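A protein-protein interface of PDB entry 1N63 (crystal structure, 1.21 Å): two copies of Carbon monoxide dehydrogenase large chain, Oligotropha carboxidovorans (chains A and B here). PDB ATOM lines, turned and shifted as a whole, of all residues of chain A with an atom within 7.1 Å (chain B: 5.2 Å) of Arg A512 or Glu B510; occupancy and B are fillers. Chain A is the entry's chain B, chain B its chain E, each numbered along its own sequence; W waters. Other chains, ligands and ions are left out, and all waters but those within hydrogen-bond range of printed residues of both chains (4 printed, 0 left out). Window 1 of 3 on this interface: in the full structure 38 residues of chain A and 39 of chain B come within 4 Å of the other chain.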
ATOM      1  N   GLU A 510     -10.556 -14.742   0.742  1.00  0.00           N
ATOM      2  CA  GLU A 510     -10.965 -15.825   1.649  1.00  0.00           C
ATOM      3  C   GLU A 510     -11.955 -15.224   2.659  1.00  0.00           C
ATOM      4  O   GLU A 510     -11.658 -14.168   3.243  1.00  0.00           O
ATOM      5  CB  GLU A 510      -9.706 -16.388   2.371  1.00  0.00           C
ATOM      6  CG  GLU A 510     -10.142 -17.532   3.300  1.00  0.00           C
ATOM      7  CD  GLU A 510      -9.066 -18.483   3.771  1.00  0.00           C
ATOM      8  OE1 GLU A 510      -7.915 -18.083   3.857  1.00  0.00           O
ATOM      9  OE2 GLU A 510      -9.424 -19.652   4.000  1.00  0.00           O
ATOM     10  N   ILE A 511     -13.109 -15.863   2.849  1.00  0.00           N
ATOM     11  CA  ILE A 511     -14.181 -15.363   3.703  1.00  0.00           C
ATOM     12  C   ILE A 511     -14.539 -16.472   4.640  1.00  0.00           C
ATOM     13  O   ILE A 511     -14.939 -17.555   4.208  1.00  0.00           O
ATOM     14  CB  ILE A 511     -15.376 -14.998   2.845  1.00  0.00           C
ATOM     15  CG1 ILE A 511     -15.039 -13.999   1.744  1.00  0.00           C
ATOM     16  CG2 ILE A 511     -16.481 -14.467   3.749  1.00  0.00           C
ATOM     17  CD1 ILE A 511     -16.154 -13.635   0.816  1.00  0.00           C
ATOM     18  N   ARG A 512     -14.588 -16.176   5.939  1.00  0.00           N
ATOM     19  CA  ARG A 512     -14.933 -17.141   6.959  1.00  0.00           C
ATOM     20  C   ARG A 512     -16.032 -16.551   7.863  1.00  0.00           C
ATOM     21  O   ARG A 512     -15.873 -15.479   8.409  1.00  0.00           O
ATOM     22  CB  ARG A 512     -13.682 -17.498   7.779  1.00  0.00           C
ATOM     23  CG  ARG A 512     -14.007 -18.462   8.916  1.00  0.00           C
ATOM     24  CD  ARG A 512     -12.718 -18.872   9.659  1.00  0.00           C
ATOM     25  NE  ARG A 512     -11.983 -19.806   8.802  1.00  0.00           N
ATOM     26  CZ  ARG A 512     -10.719 -19.697   8.432  1.00  0.00           C
ATOM     27  NH1 ARG A 512      -9.938 -18.785   8.975  1.00  0.00           N
ATOM     28  NH2 ARG A 512     -10.233 -20.481   7.471  1.00  0.00           N
ATOM     29  N   ILE A 513     -17.167 -17.269   7.965  1.00  0.00           N
ATOM     30  CA  ILE A 513     -18.283 -16.827   8.806  1.00  0.00           C
ATOM     31  C   ILE A 513     -18.168 -17.540  10.157  1.00  0.00           C
ATOM     32  O   ILE A 513     -18.068 -18.768  10.195  1.00  0.00           O
ATOM     33  CB  ILE A 513     -19.647 -17.186   8.177  1.00  0.00           C
ATOM     34  CG1 ILE A 513     -19.680 -16.998   6.656  1.00  0.00           C
ATOM     35  CG2 ILE A 513     -20.752 -16.390   8.854  1.00  0.00           C
ATOM     36  CD1 ILE A 513     -19.537 -15.569   6.179  1.00  0.00           C
ATOM     37  N   HIS A 514     -18.263 -16.803  11.242  1.00  0.00           N
ATOM     38  CA  HIS A 514     -18.164 -17.332  12.577  1.00  0.00           C
ATOM     39  C   HIS A 514     -19.521 -17.888  13.016  1.00  0.00           C
ATOM     40  O   HIS A 514     -20.554 -17.583  12.424  1.00  0.00           O
ATOM     41  CB  HIS A 514     -17.687 -16.249  13.525  1.00  0.00           C
ATOM     42  CG  HIS A 514     -16.384 -15.661  13.131  1.00  0.00           C
ATOM     43  ND1 HIS A 514     -15.343 -16.498  12.789  1.00  0.00           N
ATOM     44  CD2 HIS A 514     -15.853 -14.419  13.283  1.00  0.00           C
ATOM     45  CE1 HIS A 514     -14.257 -15.772  12.632  1.00  0.00           C
ATOM     46  NE2 HIS A 514     -14.527 -14.514  12.904  1.00  0.00           N
ATOM     47  N   GLY A 517     -22.211 -15.357  13.340  1.00  0.00           N
ATOM     48  CA  GLY A 517     -22.646 -14.658  12.159  1.00  0.00           C
ATOM     49  C   GLY A 517     -21.810 -13.486  11.698  1.00  0.00           C
ATOM     50  O   GLY A 517     -22.146 -12.907  10.659  1.00  0.00           O
ATOM     51  N   SER A 518     -20.772 -13.139  12.449  1.00  0.00           N
ATOM     52  CA  SER A 518     -19.819 -12.146  11.976  1.00  0.00           C
ATOM     53  C   SER A 518     -18.765 -12.855  11.131  1.00  0.00           C
ATOM     54  O   SER A 518     -18.814 -14.046  10.942  1.00  0.00           O
ATOM     55  CB  SER A 518     -19.209 -11.396  13.138  1.00  0.00           C
ATOM     56  OG  SER A 518     -18.586 -12.270  14.044  1.00  0.00           O
ATOM     57  N   VAL A 519     -17.911 -12.064  10.484  1.00  0.00           N
ATOM     58  CA  VAL A 519     -17.051 -12.545   9.374  1.00  0.00           C
ATOM     59  C   VAL A 519     -15.675 -11.939   9.465  1.00  0.00           C
ATOM     60  O   VAL A 519     -15.486 -10.751   9.764  1.00  0.00           O
ATOM     61  CB  VAL A 519     -17.696 -12.068   8.022  1.00  0.00           C
ATOM     62  CG1 VAL A 519     -16.865 -12.521   6.855  1.00  0.00           C
ATOM     63  CG2 VAL A 519     -19.170 -12.482   7.911  1.00  0.00           C
ATOM     64  N   ILE A 520     -14.705 -12.776   9.139  1.00  0.00           N
ATOM     65  CA  ILE A 520     -13.315 -12.351   8.832  1.00  0.00           C
ATOM     66  C   ILE A 520     -13.031 -12.664   7.393  1.00  0.00           C
ATOM     67  O   ILE A 520     -13.283 -13.786   6.938  1.00  0.00           O
ATOM     68  CB  ILE A 520     -12.243 -12.925   9.790  1.00  0.00           C
ATOM     69  CG1 ILE A 520     -10.823 -12.465   9.401  1.00  0.00           C
ATOM     70  CG2 ILE A 520     -12.280 -14.402   9.846  1.00  0.00           C
ATOM     71  CD1 ILE A 520     -10.503 -11.071   9.530  1.00  0.00           C
ATOM     72  N   ALA A 521     -12.599 -11.697   6.638  1.00  0.00           N
ATOM     73  CA  ALA A 521     -12.274 -11.871   5.220  1.00  0.00           C
ATOM     74  C   ALA A 521     -10.963 -11.188   4.915  1.00  0.00           C
ATOM     75  O   ALA A 521     -10.644 -10.102   5.424  1.00  0.00           O
ATOM     76  CB  ALA A 521     -13.373 -11.318   4.336  1.00  0.00           C
ATOM     77  N   ARG A 522     -10.172 -11.831   4.058  1.00  0.00           N
ATOM     78  CA  ARG A 522      -8.870 -11.343   3.629  1.00  0.00           C
ATOM     79  C   ARG A 522      -8.736 -11.457   2.131  1.00  0.00           C
ATOM     80  O   ARG A 522      -9.303 -12.316   1.510  1.00  0.00           O
ATOM     81  CB  ARG A 522      -7.706 -12.044   4.327  1.00  0.00           C
ATOM     82  CG  ARG A 522      -7.837 -12.046   5.844  1.00  0.00           C
ATOM     83  CD  ARG A 522      -6.541 -12.486   6.501  1.00  0.00           C
ATOM     84  NE  ARG A 522      -6.578 -12.375   7.943  1.00  0.00           N
ATOM     85  CZ  ARG A 522      -7.075 -13.287   8.746  1.00  0.00           C
ATOM     86  NH1 ARG A 522      -7.457 -14.479   8.290  1.00  0.00           N
ATOM     87  NH2 ARG A 522      -7.018 -13.072  10.046  1.00  0.00           N
ATOM     88  N   THR A 560      -1.185 -14.620   6.448  1.00  0.00           N
ATOM     89  CA  THR A 560      -2.604 -14.812   6.683  1.00  0.00           C
ATOM     90  C   THR A 560      -3.472 -14.566   5.461  1.00  0.00           C
ATOM     91  O   THR A 560      -4.468 -15.253   5.266  1.00  0.00           O
ATOM     92  CB  THR A 560      -3.081 -13.921   7.859  1.00  0.00           C
ATOM     93  OG1 THR A 560      -3.024 -12.516   7.495  1.00  0.00           O
ATOM     94  CG2 THR A 560      -2.223 -14.064   9.121  1.00  0.00           C
ATOM     95  N   ILE A 587     -20.183 -19.465  -0.542  1.00  0.00           N
ATOM     96  CA  ILE A 587     -20.838 -19.551   0.759  1.00  0.00           C
ATOM     97  C   ILE A 587     -22.355 -19.516   0.662  1.00  0.00           C
ATOM     98  O   ILE A 587     -23.033 -20.315   1.293  1.00  0.00           O
ATOM     99  CB  ILE A 587     -20.330 -18.377   1.657  1.00  0.00           C
ATOM    100  CG1 ILE A 587     -18.891 -18.595   2.102  1.00  0.00           C
ATOM    101  CG2 ILE A 587     -21.282 -18.202   2.831  1.00  0.00           C
ATOM    102  CD1 ILE A 587     -18.279 -17.342   2.713  1.00  0.00           C
ATOM    103  N   TYR A 633     -22.438 -24.881  12.095  1.00  0.00           N
ATOM    104  CA  TYR A 633     -21.614 -25.321  13.218  1.00  0.00           C
ATOM    105  C   TYR A 633     -22.401 -26.292  14.138  1.00  0.00           C
ATOM    106  O   TYR A 633     -21.783 -27.176  14.749  1.00  0.00           O
ATOM    107  CB  TYR A 633     -21.075 -24.114  14.002  1.00  0.00           C
ATOM    108  CG  TYR A 633     -20.029 -23.281  13.279  1.00  0.00           C
ATOM    109  CD1 TYR A 633     -20.397 -22.248  12.483  1.00  0.00           C
ATOM    110  CD2 TYR A 633     -18.655 -23.547  13.424  1.00  0.00           C
ATOM    111  CE1 TYR A 633     -19.465 -21.469  11.830  1.00  0.00           C
ATOM    112  CE2 TYR A 633     -17.699 -22.764  12.814  1.00  0.00           C
ATOM    113  CZ  TYR A 633     -18.107 -21.730  11.992  1.00  0.00           C
ATOM    114  OH  TYR A 633     -17.136 -20.891  11.461  1.00  0.00           O
ATOM    115  N   LEU A 644     -18.682 -22.599   7.533  1.00  0.00           N
ATOM    116  CA  LEU A 644     -19.240 -21.810   6.462  1.00  0.00           C
ATOM    117  C   LEU A 644     -18.179 -20.816   6.024  1.00  0.00           C
ATOM    118  O   LEU A 644     -18.009 -19.760   6.631  1.00  0.00           O
ATOM    119  CB  LEU A 644     -20.533 -21.155   6.916  1.00  0.00           C
ATOM    120  CG  LEU A 644     -21.349 -20.530   5.812  1.00  0.00           C
ATOM    121  CD1 LEU A 644     -21.772 -21.483   4.766  1.00  0.00           C
ATOM    122  CD2 LEU A 644     -22.622 -19.870   6.387  1.00  0.00           C
ATOM    123  N   GLU A 645     -17.393 -21.201   4.997  1.00  0.00           N
ATOM    124  CA  GLU A 645     -16.293 -20.375   4.533  1.00  0.00           C
ATOM    125  C   GLU A 645     -16.015 -20.678   3.086  1.00  0.00           C
ATOM    126  O   GLU A 645     -16.393 -21.757   2.609  1.00  0.00           O
ATOM    127  CB  GLU A 645     -15.103 -20.535   5.448  1.00  0.00           C
ATOM    128  CG  GLU A 645     -14.557 -21.942   5.550  1.00  0.00           C
ATOM    129  CD  GLU A 645     -13.414 -21.973   6.525  1.00  0.00           C
ATOM    130  OE1 GLU A 645     -13.660 -21.768   7.758  1.00  0.00           O
ATOM    131  OE2 GLU A 645     -12.267 -22.016   6.037  1.00  0.00           O
ATOM    132  N   ALA A 646     -15.235 -19.830   2.448  1.00  0.00           N
ATOM    133  CA  ALA A 646     -14.821 -20.098   1.087  1.00  0.00           C
ATOM    134  C   ALA A 646     -13.645 -19.250   0.683  1.00  0.00           C
ATOM    135  O   ALA A 646     -13.387 -18.164   1.225  1.00  0.00           O
ATOM    136  CB  ALA A 646     -15.954 -19.906   0.082  1.00  0.00           C
ATOM    137  N   VAL A 647     -12.924 -19.729  -0.329  1.00  0.00           N
ATOM    138  CA  VAL A 647     -11.844 -19.020  -0.978  1.00  0.00           C
ATOM    139  C   VAL A 647     -12.105 -19.001  -2.486  1.00  0.00           C
ATOM    140  O   VAL A 647     -12.690 -19.946  -3.020  1.00  0.00           O
ATOM    141  CB  VAL A 647     -10.475 -19.638  -0.712  1.00  0.00           C
ATOM    142  CG1 VAL A 647     -10.196 -19.684   0.762  1.00  0.00           C
ATOM    143  CG2 VAL A 647     -10.398 -20.981  -1.304  1.00  0.00           C
ATOM    144  N   SER B 508     -10.520 -29.142  12.428  1.00  0.00           N
ATOM    145  CA  SER B 508     -10.266 -28.560  11.145  1.00  0.00           C
ATOM    146  C   SER B 508      -8.788 -28.348  10.842  1.00  0.00           C
ATOM    147  O   SER B 508      -7.964 -28.266  11.727  1.00  0.00           O
ATOM    148  CB  SER B 508     -10.979 -27.214  11.080  1.00  0.00           C
ATOM    149  OG  SER B 508     -10.406 -26.347  12.047  1.00  0.00           O
ATOM    150  N   ALA B 509      -8.503 -28.240   9.542  1.00  0.00           N
ATOM    151  CA  ALA B 509      -7.174 -27.925   9.031  1.00  0.00           C
ATOM    152  C   ALA B 509      -7.305 -27.098   7.768  1.00  0.00           C
ATOM    153  O   ALA B 509      -8.180 -27.355   6.928  1.00  0.00           O
ATOM    154  CB  ALA B 509      -6.392 -29.254   8.701  1.00  0.00           C
ATOM    155  N   GLU B 510      -6.397 -26.143   7.605  1.00  0.00           N
ATOM    156  CA  GLU B 510      -6.266 -25.344   6.366  1.00  0.00           C
ATOM    157  C   GLU B 510      -4.781 -25.432   5.983  1.00  0.00           C
ATOM    158  O   GLU B 510      -3.919 -25.195   6.787  1.00  0.00           O
ATOM    159  CB  GLU B 510      -6.716 -23.892   6.597  1.00  0.00           C
ATOM    160  CG  GLU B 510      -6.492 -23.081   5.331  1.00  0.00           C
ATOM    161  CD  GLU B 510      -7.294 -21.785   5.301  1.00  0.00           C
ATOM    162  OE1 GLU B 510      -7.563 -21.197   6.374  1.00  0.00           O
ATOM    163  OE2 GLU B 510      -7.741 -21.409   4.182  1.00  0.00           O
ATOM    164  N   ILE B 511      -4.539 -25.775   4.736  1.00  0.00           N
ATOM    165  CA  ILE B 511      -3.171 -25.946   4.222  1.00  0.00           C
ATOM    166  C   ILE B 511      -3.018 -25.121   2.958  1.00  0.00           C
ATOM    167  O   ILE B 511      -3.849 -25.228   2.067  1.00  0.00           O
ATOM    168  CB  ILE B 511      -2.961 -27.414   3.884  1.00  0.00           C
ATOM    169  CG1 ILE B 511      -3.176 -28.334   5.072  1.00  0.00           C
ATOM    170  CG2 ILE B 511      -1.551 -27.587   3.270  1.00  0.00           C
ATOM    171  CD1 ILE B 511      -3.122 -29.816   4.728  1.00  0.00           C
ATOM    172  N   ARG B 512      -1.993 -24.255   2.905  1.00  0.00           N
ATOM    173  CA  ARG B 512      -1.744 -23.431   1.749  1.00  0.00           C
ATOM    174  C   ARG B 512      -0.331 -23.640   1.297  1.00  0.00           C
ATOM    175  O   ARG B 512       0.622 -23.471   2.075  1.00  0.00           O
ATOM    176  CB  ARG B 512      -1.925 -21.955   2.131  1.00  0.00           C
ATOM    177  CG  ARG B 512      -1.660 -20.947   1.059  1.00  0.00           C
ATOM    178  CD  ARG B 512      -1.992 -19.502   1.490  1.00  0.00           C
ATOM    179  NE  ARG B 512      -3.459 -19.350   1.434  1.00  0.00           N
ATOM    180  CZ  ARG B 512      -4.226 -19.028   2.457  1.00  0.00           C
ATOM    181  NH1 ARG B 512      -3.687 -18.297   3.457  1.00  0.00           N
ATOM    182  NH2 ARG B 512      -5.545 -19.076   2.330  1.00  0.00           N
ATOM    183  N   ILE B 520       2.134 -23.178   4.655  1.00  0.00           N
ATOM    184  CA  ILE B 520       1.595 -22.754   5.955  1.00  0.00           C
ATOM    185  C   ILE B 520       0.320 -23.569   6.170  1.00  0.00           C
ATOM    186  O   ILE B 520      -0.546 -23.601   5.294  1.00  0.00           O
ATOM    187  CB  ILE B 520       1.385 -21.221   6.011  1.00  0.00           C
ATOM    188  CG1 ILE B 520       0.717 -20.822   7.311  1.00  0.00           C
ATOM    189  CG2 ILE B 520       0.535 -20.663   4.883  1.00  0.00           C
ATOM    190  CD1 ILE B 520       1.544 -21.058   8.511  1.00  0.00           C
ATOM    191  N   ALA B 521       0.213 -24.144   7.363  1.00  0.00           N
ATOM    192  CA  ALA B 521      -0.946 -24.943   7.713  1.00  0.00           C
ATOM    193  C   ALA B 521      -1.349 -24.593   9.127  1.00  0.00           C
ATOM    194  O   ALA B 521      -0.506 -24.374  10.005  1.00  0.00           O
ATOM    195  CB  ALA B 521      -0.673 -26.449   7.575  1.00  0.00           C
ATOM    196  N   ARG B 522      -2.655 -24.507   9.351  1.00  0.00           N
ATOM    197  CA  ARG B 522      -3.208 -24.210  10.662  1.00  0.00           C
ATOM    198  C   ARG B 522      -4.354 -25.160  10.956  1.00  0.00           C
ATOM    199  O   ARG B 522      -5.041 -25.640  10.058  1.00  0.00           O
ATOM    200  CB  ARG B 522      -3.742 -22.782  10.696  1.00  0.00           C
ATOM    201  CG  ARG B 522      -2.663 -21.744  10.337  1.00  0.00           C
ATOM    202  CD  ARG B 522      -3.123 -20.371  10.735  1.00  0.00           C
ATOM    203  NE  ARG B 522      -2.091 -19.386  10.557  1.00  0.00           N
ATOM    204  CZ  ARG B 522      -1.831 -18.777   9.429  1.00  0.00           C
ATOM    205  NH1 ARG B 522      -2.661 -18.874   8.414  1.00  0.00           N
ATOM    206  NH2 ARG B 522      -0.837 -17.898   9.385  1.00  0.00           N
ATOM    207  N   MET B 523      -4.569 -25.374  12.243  1.00  0.00           N
ATOM    208  CA  MET B 523      -5.518 -26.368  12.714  1.00  0.00           C
ATOM    209  C   MET B 523      -6.303 -25.753  13.861  1.00  0.00           C
ATOM    210  O   MET B 523      -5.827 -24.787  14.480  1.00  0.00           O
ATOM    211  CB  MET B 523      -4.873 -27.650  13.193  1.00  0.00           C
ATOM    212  CG  MET B 523      -4.232 -28.504  12.104  1.00  0.00           C
ATOM    213  SD  MET B 523      -2.636 -27.807  11.481  1.00  0.00           S
ATOM    214  CE  MET B 523      -2.420 -28.863  10.011  1.00  0.00           C
ATOM    215  N   ASP B 559      -8.140 -15.486  15.036  1.00  0.00           N
ATOM    216  CA  ASP B 559      -8.291 -14.731  13.803  1.00  0.00           C
ATOM    217  C   ASP B 559      -7.797 -15.530  12.587  1.00  0.00           C
ATOM    218  O   ASP B 559      -8.231 -15.287  11.473  1.00  0.00           O
ATOM    219  CB  ASP B 559      -7.490 -13.420  13.822  1.00  0.00           C
ATOM    220  CG  ASP B 559      -7.978 -12.342  14.709  1.00  0.00           C
ATOM    221  OD1 ASP B 559      -9.090 -12.395  15.264  1.00  0.00           O
ATOM    222  OD2 ASP B 559      -7.225 -11.316  14.819  1.00  0.00           O
ATOM    223  N   THR B 560      -6.841 -16.429  12.800  1.00  0.00           N
ATOM    224  CA  THR B 560      -6.105 -17.030  11.686  1.00  0.00           C
ATOM    225  C   THR B 560      -6.404 -18.547  11.511  1.00  0.00           C
ATOM    226  O   THR B 560      -6.481 -19.027  10.392  1.00  0.00           O
ATOM    227  CB  THR B 560      -4.606 -16.760  11.775  1.00  0.00           C
ATOM    228  OG1 THR B 560      -4.004 -17.501  12.853  1.00  0.00           O
ATOM    229  CG2 THR B 560      -4.266 -15.247  11.981  1.00  0.00           C
ATOM    230  N   ALA B 561      -6.382 -19.267  12.616  1.00  0.00           N
ATOM    231  CA  ALA B 561      -6.688 -20.694  12.545  1.00  0.00           C
ATOM    232  C   ALA B 561      -8.119 -20.981  12.185  1.00  0.00           C
ATOM    233  O   ALA B 561      -9.025 -20.251  12.678  1.00  0.00           O
ATOM    234  CB  ALA B 561      -6.298 -21.326  13.822  1.00  0.00           C
ATOM    235  N   PRO B 562      -8.400 -22.047  11.430  1.00  0.00           N
ATOM    236  CA  PRO B 562      -9.789 -22.419  11.188  1.00  0.00           C
ATOM    237  C   PRO B 562     -10.477 -22.782  12.493  1.00  0.00           C
ATOM    238  O   PRO B 562      -9.788 -23.106  13.465  1.00  0.00           O
ATOM    239  CB  PRO B 562      -9.695 -23.584  10.223  1.00  0.00           C
ATOM    240  CG  PRO B 562      -8.349 -24.257  10.601  1.00  0.00           C
ATOM    241  CD  PRO B 562      -7.434 -23.064  10.954  1.00  0.00           C
ATOM    242  N   TYR B 563     -11.801 -22.610  12.570  1.00  0.00           N
ATOM    243  CA  TYR B 563     -12.468 -22.910  13.811  1.00  0.00           C
ATOM    244  C   TYR B 563     -12.278 -24.355  14.170  1.00  0.00           C
ATOM    245  O   TYR B 563     -12.487 -25.236  13.355  1.00  0.00           O
ATOM    246  CB  TYR B 563     -13.973 -22.552  13.704  1.00  0.00           C
ATOM    247  CG  TYR B 563     -14.663 -22.379  15.024  1.00  0.00           C
ATOM    248  CD1 TYR B 563     -15.046 -23.460  15.789  1.00  0.00           C
ATOM    249  CD2 TYR B 563     -14.952 -21.121  15.517  1.00  0.00           C
ATOM    250  CE1 TYR B 563     -15.676 -23.312  16.992  1.00  0.00           C
ATOM    251  CE2 TYR B 563     -15.575 -20.954  16.721  1.00  0.00           C
ATOM    252  CZ  TYR B 563     -15.951 -22.046  17.458  1.00  0.00           C
ATOM    253  OH  TYR B 563     -16.579 -21.859  18.690  1.00  0.00           O
ATOM    254  N   GLU B 645      -4.374 -24.861  -2.386  1.00  0.00           N
ATOM    255  CA  GLU B 645      -4.669 -24.838  -1.005  1.00  0.00           C
ATOM    256  C   GLU B 645      -5.951 -25.608  -0.746  1.00  0.00           C
ATOM    257  O   GLU B 645      -6.737 -25.814  -1.660  1.00  0.00           O
ATOM    258  CB  GLU B 645      -4.694 -23.428  -0.487  1.00  0.00           C
ATOM    259  CG  GLU B 645      -5.721 -22.544  -1.180  1.00  0.00           C
ATOM    260  CD  GLU B 645      -5.644 -21.149  -0.634  1.00  0.00           C
ATOM    261  OE1 GLU B 645      -6.512 -20.735   0.182  1.00  0.00           O
ATOM    262  OE2 GLU B 645      -4.636 -20.434  -0.881  1.00  0.00           O
ATOM    263  N   ALA B 646      -6.227 -25.911   0.528  1.00  0.00           N
ATOM    264  CA  ALA B 646      -7.489 -26.562   0.872  1.00  0.00           C
ATOM    265  C   ALA B 646      -7.766 -26.473   2.348  1.00  0.00           C
ATOM    266  O   ALA B 646      -6.848 -26.267   3.178  1.00  0.00           O
ATOM    267  CB  ALA B 646      -7.500 -28.021   0.445  1.00  0.00           C
ATOM    268  N   VAL B 647      -9.023 -26.614   2.666  1.00  0.00           N
ATOM    269  CA  VAL B 647      -9.517 -26.646   4.024  1.00  0.00           C
ATOM    270  C   VAL B 647     -10.386 -27.915   4.180  1.00  0.00           C
ATOM    271  O   VAL B 647     -11.086 -28.322   3.236  1.00  0.00           O
ATOM    272  CB  VAL B 647     -10.362 -25.386   4.348  1.00  0.00           C
ATOM    273  CG1 VAL B 647     -10.972 -25.465   5.717  1.00  0.00           C
ATOM    274  CG2 VAL B 647      -9.605 -24.140   4.174  1.00  0.00           C
ATOM    275  N   ASN B 648     -10.366 -28.513   5.376  1.00  0.00           N
ATOM    276  CA  ASN B 648     -11.313 -29.519   5.739  1.00  0.00           C
ATOM    277  C   ASN B 648     -11.787 -29.316   7.154  1.00  0.00           C
ATOM    278  O   ASN B 648     -10.969 -29.107   8.053  1.00  0.00           O
ATOM    279  CB  ASN B 648     -10.748 -30.924   5.555  1.00  0.00           C
ATOM    280  CG  ASN B 648     -11.739 -32.045   5.965  1.00  0.00           C
ATOM    281  OD1 ASN B 648     -11.512 -32.717   6.936  1.00  0.00           O
ATOM    282  ND2 ASN B 648     -12.845 -32.158   5.246  1.00  0.00           N
ATOM    283  N   TYR B 649     -13.089 -29.380   7.349  1.00  0.00           N
ATOM    284  CA  TYR B 649     -13.696 -29.481   8.666  1.00  0.00           C
ATOM    285  C   TYR B 649     -14.242 -30.902   8.758  1.00  0.00           C
ATOM    286  O   TYR B 649     -15.114 -31.285   8.005  1.00  0.00           O
ATOM    287  CB  TYR B 649     -14.836 -28.483   8.814  1.00  0.00           C
ATOM    288  CG  TYR B 649     -14.390 -27.046   9.075  1.00  0.00           C
ATOM    289  CD1 TYR B 649     -13.483 -26.370   8.285  1.00  0.00           C
ATOM    290  CD2 TYR B 649     -14.934 -26.347  10.148  1.00  0.00           C
ATOM    291  CE1 TYR B 649     -13.080 -25.082   8.581  1.00  0.00           C
ATOM    292  CE2 TYR B 649     -14.553 -25.040  10.444  1.00  0.00           C
ATOM    293  CZ  TYR B 649     -13.614 -24.427   9.681  1.00  0.00           C
ATOM    294  OH  TYR B 649     -13.286 -23.097   9.978  1.00  0.00           O
HETATM  295  O   HOH W   1     -10.238 -17.982  11.868  1.00  0.00           O
HETATM  296  O   HOH W   2      -5.173 -17.967   5.995  1.00  0.00           O
HETATM  297  O   HOH W   3     -16.230 -21.988   8.911  1.00  0.00           O
HETATM  298  O   HOH W   4      -7.278 -17.598   8.173  1.00  0.00           O
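The backbone NH (N) of Arg A512 sits at hydrogen-bond distance from the backbone carbonyl oxygen (O) of Ile A520 (2.9 Å). The backbone carbonyl oxygen of Ile A513 lies within hydrogen-bond range of the side-chain hydroxyl of Tyr A633, at 2.6 Å. N of Tyr B563 is in hydrogen-bond range of OH of Tyr B649 (3.0 Å). The backbone carbonyl oxygen (O) of Arg A522 sits at hydrogen-bond distance from the backbone NH (N) of Glu A510 (2.8 Å). NE of Arg B512 is in salt-bridge range of OE2 of Glu B645 (2.8 Å). The backbone NH (N) of Arg B512 sits at hydrogen-bond distance from the backbone carbonyl oxygen (O) of Ile B520 (2.9 Å).
The backbone carbonyl oxygen (O) of Asp B559 sits at hydrogen-bond distance from the guanidinium group (NH2) of Arg A522. NH2 of Arg A512 is in salt-bridge range of OE1 of Glu B510 (3.0 Å). OE1 of Glu A510 is in salt-bridge range of NH2 of Arg B512 (3.0 Å). OE2 of Glu A510 lies close to OE2 of Glu B510 (2.4 Å). The side-chain hydroxyl (OH) of Tyr B649 is in hydrogen-bond range of the side-chain carboxylate (OE1) of Glu A645 (2.6 Å).
Of the 18 printed residues of chain A, 7 touch a printed residue of chain B. Printed residues of chain A that touch a printed residue of chain B: Glu A510, Arg A512, Arg A522, Thr A560, Tyr A633, Glu A645 and Val A647. Hydrophobic or aromatic side chains of chain A within 4 Å of the printed part of chain B: Tyr A633 and Val A647. Hydrophobic or aromatic side chains of chain B within 4 Å of the printed part of chain A: Tyr B563, Val B647 and Tyr B649. Among the printed residues, 13 pairs touch across the chains. Among the printed residues, Asp or Glu carboxylates within 4 Å of a Lys or Arg side-chain nitrogen of the other chain: Glu A510 with Arg B512 (3.0 Å) and Arg A512 with Glu B510 (3.0 Å).
Among the printed residues, merely in contact across the chains: Arg A512 with Thr B560 (3.7 Å), Arg A512 with Pro B562 (3.98 Å), Arg A512 with Tyr B649 (3.7 Å), Thr A560 with Arg B512 (3.6 Å), Thr A560 with Thr B560 (3.7 Å), Tyr A633 with Tyr B563 (3.8 Å), Glu A645 with Val B647 (3.7 Å) and Val A647 with Glu B645 (3.9 Å).
Water W1 lies within hydrogen-bond range of O of Ala B561, NH1 of Arg A512 and O of Asp B559. Water W4 lies within hydrogen-bond range of the backbone carbonyl oxygen (O) of Thr B560, the guanidinium group (NH1) of Arg A512 and the guanidinium group (NH1) of Arg A522. Water W3 lies within hydrogen-bond range of OE1 of Glu A645 (2.8 Å), N of Leu A644 (2.9 Å), OH of Tyr A633 (2.9 Å) and OH of Tyr B649 (3.3 Å). Water W2 lies within hydrogen-bond range of O of Thr A560, NH1 of Arg B512 and OE1 of Glu A510.
Of the printed residues of chain B, Arg A512 touches Glu B510, Thr B560, Pro B562 and Tyr B649. Printed residues of chain A within 4 Å of Glu B510: Glu A510 (2.4 Å) and Arg A512 (3.0 Å). Printed residues of chain B within 4 Å of Tyr A633: Tyr B563 (3.8 Å). Of the printed residues of chain A, Tyr B563 touches Tyr A633 (3.8 Å). Of the printed residues of chain A, Val B647 touches Glu A645 (3.7 Å). Of the printed residues of chain A, Pro B562 touches Arg A512. Ile B511 touches none of the printed residues of chain A. The nearest printed residue of chain B that does not touch Arg A512 is Ala B561 (4.1 Å). The nearest printed residue of chain B that does not touch Glu A645 is Glu B510 (4.8 Å).
Glu B510 touches its own counterpart, Glu A510. Glu A510 touches Arg B512, and with the chains exchanged Arg A512 touches Glu B510. Arg A512 touches Thr B560, and with the chains exchanged Thr A560 touches Arg B512. Thr A560 touches its own counterpart, Thr B560. 10 positions are printed for both chains. Of the 13 pairs that touch across the chains among the printed residues, 8 have their exchanged pair printed and touching as well.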
